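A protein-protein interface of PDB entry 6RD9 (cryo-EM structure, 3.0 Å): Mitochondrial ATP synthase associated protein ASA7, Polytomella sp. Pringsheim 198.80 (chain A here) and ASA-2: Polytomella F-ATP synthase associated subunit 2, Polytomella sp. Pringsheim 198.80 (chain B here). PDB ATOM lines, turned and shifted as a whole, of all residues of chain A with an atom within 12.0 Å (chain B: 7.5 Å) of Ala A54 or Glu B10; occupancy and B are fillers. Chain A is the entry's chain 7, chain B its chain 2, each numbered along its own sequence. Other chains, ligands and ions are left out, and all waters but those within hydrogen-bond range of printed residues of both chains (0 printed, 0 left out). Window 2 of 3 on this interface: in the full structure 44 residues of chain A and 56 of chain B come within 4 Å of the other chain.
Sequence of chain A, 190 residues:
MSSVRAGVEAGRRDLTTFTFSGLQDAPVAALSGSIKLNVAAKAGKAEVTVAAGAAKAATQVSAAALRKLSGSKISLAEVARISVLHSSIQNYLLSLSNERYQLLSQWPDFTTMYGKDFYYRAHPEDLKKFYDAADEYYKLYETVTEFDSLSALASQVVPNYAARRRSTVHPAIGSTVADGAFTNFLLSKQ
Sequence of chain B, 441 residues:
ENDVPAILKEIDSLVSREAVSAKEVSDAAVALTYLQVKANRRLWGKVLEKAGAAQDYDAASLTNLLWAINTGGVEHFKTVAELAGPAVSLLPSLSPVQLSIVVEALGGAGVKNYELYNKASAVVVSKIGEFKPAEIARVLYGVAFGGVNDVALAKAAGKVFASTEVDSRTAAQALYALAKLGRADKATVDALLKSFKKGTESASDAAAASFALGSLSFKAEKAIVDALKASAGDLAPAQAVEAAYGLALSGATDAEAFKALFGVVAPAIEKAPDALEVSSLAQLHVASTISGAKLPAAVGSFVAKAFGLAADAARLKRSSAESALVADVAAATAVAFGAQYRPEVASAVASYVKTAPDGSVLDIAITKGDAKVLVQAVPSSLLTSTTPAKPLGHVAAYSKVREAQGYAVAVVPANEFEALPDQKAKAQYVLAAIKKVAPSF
CB of Ser A34 touches CD1 of Leu B14 (3.7 Å). CG2 of Val A50 touches CD1 of Ile B7, at 3.6 Å. Ala A51 touches Ile B7. CD1 of Ile B7 touches N of Ala A52, 3.6 Å away. O of Ala A52 touches CB of Glu B10 (3.3 Å). Glu B10 touches Ala A54 (OE2 to N, 3.8 Å). CB of Ala A55 touches O of Ala B6 (3.7 Å). Ile B7 touches Ala A55 (CG1 to CB, 3.8 Å). Ala A57 touches Asp B3. CD1 of Ile B7 touches N of Ala A57, 3.997 Å away.
The backbone carbonyl oxygen (O) of Ala A57 is in hydrogen-bond range of the backbone NH (N) of Val A50 (2.8 Å). N of Lys A36 lies within hydrogen-bond range of O of Ala A51 (2.6 Å). OG of Ser A32 sits at hydrogen-bond distance from N of Ser A34 (3.3 Å).
O of Glu B1 lies close to O of Lys A56, at 3.1 Å. N of Asp B3 sits at hydrogen-bond distance from O of Lys A56, 2.7 Å away. OG of Ser A34 sits at hydrogen-bond distance from NH2 of Arg B17 (3.5 Å).
Printed residues of chain A that touch a printed residue of chain B: Ser A34, Ile A35, Val A50, Ala A51, Ala A52, Gly A53, Ala A54, Ala A55, Lys A56 and Ala A57. Hydrophobic or aromatic side chains of chain A within 4 Å of the printed part of chain B: Ile A35, Val A50, Ala A52, Ala A55 and Ala A57. Of the 16 printed residues of chain B, 8 touch a printed residue of chain A. Hydrophobic or aromatic side chains of chain B that line the printed part of chain A: Ile B7, Ile B11 and Leu B14. Among the printed residues, 15 pairs touch across the chains. Among the printed residues, no Asp or Glu carboxylate lies within 4 Å of a Lys or Arg side-chain nitrogen of the other chain.
Gly A33 touches none of the printed residues of chain B. Of the printed residues of chain B, Ala A51 touches Ile B7 (3.98 Å). Printed residues of chain B within 4 Å of Ala A52: Ile B7 (3.6 Å) and Glu B10 (3.3 Å). Ala A54 touches one residue of chain B. Of the printed residues of chain B, Ala A55 touches Ala B6 (3.7 Å) and Ile B7 (3.8 Å). Of the printed residues of chain A, Asp B3 touches Lys A56 (2.7 Å) and Ala A57 (3.4 Å). Of chain A, only Ala A55 comes within 4 Å of Ala B6. Lys B9 touches none of the printed residues of chain A. Glu B10 touches just these residues of chain A: Ala A52, Gly A53 and Ala A54. Ile B11 touches just one residue of chain A: Ile A35 (3.9 Å). No residue of chain A comes within 4 Å of Asp B12. Of the printed residues of chain A, Leu B14 touches Ser A34 (3.7 Å).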
ATOM      1  N   SER A  32     -10.000  10.943  24.275  1.00  0.00           N
ATOM      2  CA  SER A  32      -9.523  10.132  25.373  1.00  0.00           C
ATOM      3  C   SER A  32      -8.120   9.632  25.062  1.00  0.00           C
ATOM      4  O   SER A  32      -7.473  10.070  24.107  1.00  0.00           O
ATOM      5  CB  SER A  32     -10.462   8.960  25.617  1.00  0.00           C
ATOM      6  OG  SER A  32     -10.359   8.041  24.551  1.00  0.00           O
ATOM      7  N   GLY A  33      -7.639   8.710  25.883  1.00  0.00           N
ATOM      8  CA  GLY A  33      -6.413   8.007  25.590  1.00  0.00           C
ATOM      9  C   GLY A  33      -6.677   6.528  25.446  1.00  0.00           C
ATOM     10  O   GLY A  33      -5.789   5.760  25.072  1.00  0.00           O
ATOM     11  N   SER A  34      -7.912   6.124  25.737  1.00  0.00           N
ATOM     12  CA  SER A  34      -8.268   4.713  25.670  1.00  0.00           C
ATOM     13  C   SER A  34      -8.336   4.226  24.237  1.00  0.00           C
ATOM     14  O   SER A  34      -8.218   3.025  23.979  1.00  0.00           O
ATOM     15  CB  SER A  34      -9.606   4.481  26.359  1.00  0.00           C
ATOM     16  OG  SER A  34      -9.545   4.828  27.725  1.00  0.00           O
ATOM     17  N   ILE A  35      -8.531   5.142  23.301  1.00  0.00           N
ATOM     18  CA  ILE A  35      -8.618   4.832  21.883  1.00  0.00           C
ATOM     19  C   ILE A  35      -8.030   6.009  21.128  1.00  0.00           C
ATOM     20  O   ILE A  35      -8.325   7.165  21.438  1.00  0.00           O
ATOM     21  CB  ILE A  35     -10.075   4.521  21.486  1.00  0.00           C
ATOM     22  CG1 ILE A  35     -10.234   4.354  19.987  1.00  0.00           C
ATOM     23  CG2 ILE A  35     -11.045   5.536  22.054  1.00  0.00           C
ATOM     24  CD1 ILE A  35     -11.543   3.713  19.653  1.00  0.00           C
ATOM     25  N   LYS A  36      -7.134   5.730  20.194  1.00  0.00           N
ATOM     26  CA  LYS A  36      -6.397   6.778  19.505  1.00  0.00           C
ATOM     27  C   LYS A  36      -6.905   6.887  18.079  1.00  0.00           C
ATOM     28  O   LYS A  36      -6.779   5.943  17.292  1.00  0.00           O
ATOM     29  CB  LYS A  36      -4.896   6.506  19.544  1.00  0.00           C
ATOM     30  CG  LYS A  36      -4.246   6.955  20.846  1.00  0.00           C
ATOM     31  CD  LYS A  36      -2.831   6.436  20.985  1.00  0.00           C
ATOM     32  CE  LYS A  36      -2.815   4.942  21.241  1.00  0.00           C
ATOM     33  NZ  LYS A  36      -3.602   4.576  22.450  1.00  0.00           N
ATOM     34  N   THR A  49      -7.104   6.575  11.018  1.00  0.00           N
ATOM     35  CA  THR A  49      -6.242   5.610  11.687  1.00  0.00           C
ATOM     36  C   THR A  49      -6.760   5.458  13.104  1.00  0.00           C
ATOM     37  O   THR A  49      -6.682   6.398  13.902  1.00  0.00           O
ATOM     38  CB  THR A  49      -4.787   6.066  11.680  1.00  0.00           C
ATOM     39  OG1 THR A  49      -4.303   6.087  10.332  1.00  0.00           O
ATOM     40  CG2 THR A  49      -3.936   5.126  12.501  1.00  0.00           C
ATOM     41  N   VAL A  50      -7.313   4.295  13.409  1.00  0.00           N
ATOM     42  CA  VAL A  50      -7.850   4.028  14.732  1.00  0.00           C
ATOM     43  C   VAL A  50      -6.947   3.031  15.442  1.00  0.00           C
ATOM     44  O   VAL A  50      -6.333   2.151  14.828  1.00  0.00           O
ATOM     45  CB  VAL A  50      -9.312   3.540  14.664  1.00  0.00           C
ATOM     46  CG1 VAL A  50     -10.162   4.556  13.971  1.00  0.00           C
ATOM     47  CG2 VAL A  50      -9.403   2.299  13.872  1.00  0.00           C
ATOM     48  N   ALA A  51      -6.844   3.201  16.756  1.00  0.00           N
ATOM     49  CA  ALA A  51      -5.943   2.399  17.573  1.00  0.00           C
ATOM     50  C   ALA A  51      -6.595   2.231  18.932  1.00  0.00           C
ATOM     51  O   ALA A  51      -6.657   3.188  19.705  1.00  0.00           O
ATOM     52  CB  ALA A  51      -4.585   3.074  17.702  1.00  0.00           C
ATOM     53  N   ALA A  52      -7.087   1.031  19.218  1.00  0.00           N
ATOM     54  CA  ALA A  52      -7.772   0.753  20.473  1.00  0.00           C
ATOM     55  C   ALA A  52      -7.166  -0.490  21.089  1.00  0.00           C
ATOM     56  O   ALA A  52      -7.243  -1.570  20.499  1.00  0.00           O
ATOM     57  CB  ALA A  52      -9.273   0.560  20.263  1.00  0.00           C
ATOM     58  N   GLY A  53      -6.580  -0.339  22.268  1.00  0.00           N
ATOM     59  CA  GLY A  53      -5.930  -1.471  22.903  1.00  0.00           C
ATOM     60  C   GLY A  53      -4.665  -1.829  22.158  1.00  0.00           C
ATOM     61  O   GLY A  53      -3.850  -0.964  21.820  1.00  0.00           O
ATOM     62  N   ALA A  54      -4.500  -3.115  21.877  1.00  0.00           N
ATOM     63  CA  ALA A  54      -3.379  -3.564  21.071  1.00  0.00           C
ATOM     64  C   ALA A  54      -3.656  -3.483  19.582  1.00  0.00           C
ATOM     65  O   ALA A  54      -2.709  -3.453  18.791  1.00  0.00           O
ATOM     66  CB  ALA A  54      -3.012  -5.004  21.434  1.00  0.00           C
ATOM     67  N   ALA A  55      -4.923  -3.428  19.187  1.00  0.00           N
ATOM     68  CA  ALA A  55      -5.287  -3.515  17.785  1.00  0.00           C
ATOM     69  C   ALA A  55      -5.128  -2.172  17.090  1.00  0.00           C
ATOM     70  O   ALA A  55      -5.121  -1.113  17.721  1.00  0.00           O
ATOM     71  CB  ALA A  55      -6.724  -4.002  17.639  1.00  0.00           C
ATOM     72  N   LYS A  56      -4.992  -2.229  15.772  1.00  0.00           N
ATOM     73  CA  LYS A  56      -4.957  -1.034  14.948  1.00  0.00           C
ATOM     74  C   LYS A  56      -5.721  -1.294  13.666  1.00  0.00           C
ATOM     75  O   LYS A  56      -5.796  -2.426  13.184  1.00  0.00           O
ATOM     76  CB  LYS A  56      -3.533  -0.604  14.607  1.00  0.00           C
ATOM     77  CG  LYS A  56      -2.957   0.435  15.537  1.00  0.00           C
ATOM     78  CD  LYS A  56      -1.500   0.707  15.213  1.00  0.00           C
ATOM     79  CE  LYS A  56      -0.602  -0.406  15.719  1.00  0.00           C
ATOM     80  NZ  LYS A  56      -0.611  -0.473  17.203  1.00  0.00           N
ATOM     81  N   ALA A  57      -6.298  -0.235  13.127  1.00  0.00           N
ATOM     82  CA  ALA A  57      -6.937  -0.300  11.830  1.00  0.00           C
ATOM     83  C   ALA A  57      -6.807   1.058  11.171  1.00  0.00           C
ATOM     84  O   ALA A  57      -6.763   2.085  11.851  1.00  0.00           O
ATOM     85  CB  ALA A  57      -8.405  -0.712  11.937  1.00  0.00           C
ATOM     86  N   ALA A  58      -6.705   1.050   9.847  1.00  0.00           N
ATOM     87  CA  ALA A  58      -6.625   2.282   9.069  1.00  0.00           C
ATOM     88  C   ALA A  58      -7.217   1.987   7.699  1.00  0.00           C
ATOM     89  O   ALA A  58      -6.682   1.160   6.958  1.00  0.00           O
ATOM     90  CB  ALA A  58      -5.194   2.788   8.958  1.00  0.00           C
ATOM     91  N   GLU B   1      -1.839  -6.710  10.725  1.00  0.00           N
ATOM     92  CA  GLU B   1      -1.749  -5.622  11.687  1.00  0.00           C
ATOM     93  C   GLU B   1      -2.869  -4.615  11.457  1.00  0.00           C
ATOM     94  O   GLU B   1      -3.174  -3.806  12.330  1.00  0.00           O
ATOM     95  CB  GLU B   1      -0.383  -4.942  11.603  1.00  0.00           C
ATOM     96  CG  GLU B   1      -0.107  -4.292  10.269  1.00  0.00           C
ATOM     97  CD  GLU B   1       1.276  -3.701  10.188  1.00  0.00           C
ATOM     98  OE1 GLU B   1       2.014  -3.785  11.190  1.00  0.00           O
ATOM     99  OE2 GLU B   1       1.626  -3.161   9.117  1.00  0.00           O
ATOM    100  N   ASP B   3      -6.381  -4.559  11.620  1.00  0.00           N
ATOM    101  CA  ASP B   3      -7.366  -5.417  12.266  1.00  0.00           C
ATOM    102  C   ASP B   3      -8.619  -4.585  12.478  1.00  0.00           C
ATOM    103  O   ASP B   3      -8.658  -3.751  13.385  1.00  0.00           O
ATOM    104  CB  ASP B   3      -6.831  -5.941  13.594  1.00  0.00           C
ATOM    105  CG  ASP B   3      -6.066  -7.237  13.448  1.00  0.00           C
ATOM    106  OD1 ASP B   3      -5.061  -7.417  14.165  1.00  0.00           O
ATOM    107  OD2 ASP B   3      -6.477  -8.086  12.635  1.00  0.00           O
ATOM    108  N   VAL B   4      -9.626  -4.764  11.630  1.00  0.00           N
ATOM    109  CA  VAL B   4     -10.917  -4.128  11.891  1.00  0.00           C
ATOM    110  C   VAL B   4     -11.852  -4.967  12.774  1.00  0.00           C
ATOM    111  O   VAL B   4     -12.387  -4.385  13.724  1.00  0.00           O
ATOM    112  CB  VAL B   4     -11.558  -3.613  10.580  1.00  0.00           C
ATOM    113  CG1 VAL B   4     -11.470  -4.586   9.416  1.00  0.00           C
ATOM    114  CG2 VAL B   4     -13.001  -3.180  10.799  1.00  0.00           C
ATOM    115  N   PRO B   5     -12.060  -6.288  12.624  1.00  0.00           N
ATOM    116  CA  PRO B   5     -12.920  -6.962  13.607  1.00  0.00           C
ATOM    117  C   PRO B   5     -12.247  -7.200  14.940  1.00  0.00           C
ATOM    118  O   PRO B   5     -12.947  -7.416  15.935  1.00  0.00           O
ATOM    119  CB  PRO B   5     -13.265  -8.296  12.930  1.00  0.00           C
ATOM    120  CG  PRO B   5     -12.801  -8.172  11.556  1.00  0.00           C
ATOM    121  CD  PRO B   5     -11.606  -7.308  11.666  1.00  0.00           C
ATOM    122  N   ALA B   6     -10.926  -7.179  14.997  1.00  0.00           N
ATOM    123  CA  ALA B   6     -10.234  -7.281  16.266  1.00  0.00           C
ATOM    124  C   ALA B   6     -10.145  -5.954  16.982  1.00  0.00           C
ATOM    125  O   ALA B   6      -9.798  -5.931  18.164  1.00  0.00           O
ATOM    126  CB  ALA B   6      -8.824  -7.838  16.069  1.00  0.00           C
ATOM    127  N   ILE B   7     -10.413  -4.848  16.293  1.00  0.00           N
ATOM    128  CA  ILE B   7     -10.540  -3.573  16.981  1.00  0.00           C
ATOM    129  C   ILE B   7     -11.981  -3.309  17.389  1.00  0.00           C
ATOM    130  O   ILE B   7     -12.228  -2.435  18.228  1.00  0.00           O
ATOM    131  CB  ILE B   7      -9.969  -2.422  16.135  1.00  0.00           C
ATOM    132  CG1 ILE B   7      -9.424  -1.339  17.043  1.00  0.00           C
ATOM    133  CG2 ILE B   7     -10.987  -1.829  15.221  1.00  0.00           C
ATOM    134  CD1 ILE B   7      -8.686  -0.297  16.332  1.00  0.00           C
ATOM    135  N   LEU B   8     -12.937  -4.057  16.847  1.00  0.00           N
ATOM    136  CA  LEU B   8     -14.291  -3.975  17.363  1.00  0.00           C
ATOM    137  C   LEU B   8     -14.392  -4.633  18.722  1.00  0.00           C
ATOM    138  O   LEU B   8     -15.130  -4.156  19.585  1.00  0.00           O
ATOM    139  CB  LEU B   8     -15.267  -4.621  16.395  1.00  0.00           C
ATOM    140  CG  LEU B   8     -15.520  -3.857  15.106  1.00  0.00           C
ATOM    141  CD1 LEU B   8     -16.635  -4.535  14.370  1.00  0.00           C
ATOM    142  CD2 LEU B   8     -15.848  -2.414  15.374  1.00  0.00           C
ATOM    143  N   LYS B   9     -13.644  -5.715  18.936  1.00  0.00           N
ATOM    144  CA  LYS B   9     -13.618  -6.369  20.237  1.00  0.00           C
ATOM    145  C   LYS B   9     -12.842  -5.543  21.253  1.00  0.00           C
ATOM    146  O   LYS B   9     -13.080  -5.653  22.456  1.00  0.00           O
ATOM    147  CB  LYS B   9     -13.022  -7.765  20.091  1.00  0.00           C
ATOM    148  CG  LYS B   9     -13.209  -8.652  21.297  1.00  0.00           C
ATOM    149  CD  LYS B   9     -12.721 -10.067  21.057  1.00  0.00           C
ATOM    150  CE  LYS B   9     -11.222 -10.154  21.135  1.00  0.00           C
ATOM    151  NZ  LYS B   9     -10.792 -11.567  21.046  1.00  0.00           N
ATOM    152  N   GLU B  10     -11.926  -4.702  20.796  1.00  0.00           N
ATOM    153  CA  GLU B  10     -11.245  -3.812  21.720  1.00  0.00           C
ATOM    154  C   GLU B  10     -12.053  -2.564  22.018  1.00  0.00           C
ATOM    155  O   GLU B  10     -11.787  -1.897  23.021  1.00  0.00           O
ATOM    156  CB  GLU B  10      -9.878  -3.432  21.169  1.00  0.00           C
ATOM    157  CG  GLU B  10      -8.854  -4.542  21.247  1.00  0.00           C
ATOM    158  CD  GLU B  10      -8.555  -4.946  22.676  1.00  0.00           C
ATOM    159  OE1 GLU B  10      -9.055  -6.002  23.123  1.00  0.00           O
ATOM    160  OE2 GLU B  10      -7.828  -4.200  23.360  1.00  0.00           O
ATOM    161  N   ILE B  11     -13.001  -2.212  21.149  1.00  0.00           N
ATOM    162  CA  ILE B  11     -13.955  -1.151  21.456  1.00  0.00           C
ATOM    163  C   ILE B  11     -15.069  -1.700  22.335  1.00  0.00           C
ATOM    164  O   ILE B  11     -15.529  -1.019  23.257  1.00  0.00           O
ATOM    165  CB  ILE B  11     -14.490  -0.534  20.150  1.00  0.00           C
ATOM    166  CG1 ILE B  11     -13.425   0.328  19.494  1.00  0.00           C
ATOM    167  CG2 ILE B  11     -15.694   0.339  20.379  1.00  0.00           C
ATOM    168  CD1 ILE B  11     -13.768   0.724  18.092  1.00  0.00           C
ATOM    169  N   ASP B  12     -15.468  -2.950  22.093  1.00  0.00           N
ATOM    170  CA  ASP B  12     -16.501  -3.598  22.889  1.00  0.00           C
ATOM    171  C   ASP B  12     -16.066  -3.737  24.338  1.00  0.00           C
ATOM    172  O   ASP B  12     -16.872  -3.545  25.246  1.00  0.00           O
ATOM    173  CB  ASP B  12     -16.829  -4.956  22.259  1.00  0.00           C
ATOM    174  CG  ASP B  12     -18.016  -5.666  22.896  1.00  0.00           C
ATOM    175  OD1 ASP B  12     -18.965  -5.980  22.148  1.00  0.00           O
ATOM    176  OD2 ASP B  12     -17.986  -6.016  24.093  1.00  0.00           O
ATOM    177  N   SER B  13     -14.798  -4.028  24.581  1.00  0.00           N
ATOM    178  CA  SER B  13     -14.317  -4.084  25.951  1.00  0.00           C
ATOM    179  C   SER B  13     -14.013  -2.715  26.528  1.00  0.00           C
ATOM    180  O   SER B  13     -13.705  -2.623  27.716  1.00  0.00           O
ATOM    181  CB  SER B  13     -13.077  -4.960  26.038  1.00  0.00           C
ATOM    182  OG  SER B  13     -13.315  -6.217  25.432  1.00  0.00           O
ATOM    183  N   LEU B  14     -14.070  -1.657  25.734  1.00  0.00           N
ATOM    184  CA  LEU B  14     -13.926  -0.325  26.300  1.00  0.00           C
ATOM    185  C   LEU B  14     -15.251   0.178  26.852  1.00  0.00           C
ATOM    186  O   LEU B  14     -15.282   0.861  27.876  1.00  0.00           O
ATOM    187  CB  LEU B  14     -13.374   0.631  25.248  1.00  0.00           C
ATOM    188  CG  LEU B  14     -13.560   2.136  25.425  1.00  0.00           C
ATOM    189  CD1 LEU B  14     -12.801   2.650  26.612  1.00  0.00           C
ATOM    190  CD2 LEU B  14     -13.127   2.866  24.187  1.00  0.00           C
ATOM    191  N   VAL B  15     -16.360  -0.157  26.192  1.00  0.00           N
ATOM    192  CA  VAL B  15     -17.670   0.302  26.623  1.00  0.00           C
ATOM    193  C   VAL B  15     -18.404  -0.728  27.450  1.00  0.00           C
ATOM    194  O   VAL B  15     -19.511  -0.449  27.909  1.00  0.00           O
ATOM    195  CB  VAL B  15     -18.540   0.722  25.424  1.00  0.00           C
ATOM    196  CG1 VAL B  15     -17.947   1.915  24.743  1.00  0.00           C
ATOM    197  CG2 VAL B  15     -18.677  -0.413  24.468  1.00  0.00           C
ATOM    198  N   ARG B  17     -16.994  -1.916  30.242  1.00  0.00           N
ATOM    199  CA  ARG B  17     -16.557  -1.792  31.614  1.00  0.00           C
ATOM    200  C   ARG B  17     -17.477  -0.823  32.346  1.00  0.00           C
ATOM    201  O   ARG B  17     -18.509  -0.402  31.830  1.00  0.00           O
ATOM    202  CB  ARG B  17     -15.089  -1.399  31.674  1.00  0.00           C
ATOM    203  CG  ARG B  17     -14.708  -0.192  30.917  1.00  0.00           C
ATOM    204  CD  ARG B  17     -13.283  -0.349  30.481  1.00  0.00           C
ATOM    205  NE  ARG B  17     -12.615   0.933  30.336  1.00  0.00           N
ATOM    206  CZ  ARG B  17     -11.405   1.073  29.817  1.00  0.00           C
ATOM    207  NH1 ARG B  17     -10.744   0.010  29.389  1.00  0.00           N
ATOM    208  NH2 ARG B  17     -10.862   2.274  29.718  1.00  0.00           N
ATOM    209  N   LEU B  43     -23.100  -3.685  19.422  1.00  0.00           N
ATOM    210  CA  LEU B  43     -21.990  -2.805  19.753  1.00  0.00           C
ATOM    211  C   LEU B  43     -22.394  -1.347  19.675  1.00  0.00           C
ATOM    212  O   LEU B  43     -21.890  -0.525  20.440  1.00  0.00           O
ATOM    213  CB  LEU B  43     -20.817  -3.082  18.827  1.00  0.00           C
ATOM    214  CG  LEU B  43     -19.536  -2.281  18.976  1.00  0.00           C
ATOM    215  CD1 LEU B  43     -19.087  -2.280  20.401  1.00  0.00           C
ATOM    216  CD2 LEU B  43     -18.502  -2.891  18.096  1.00  0.00           C
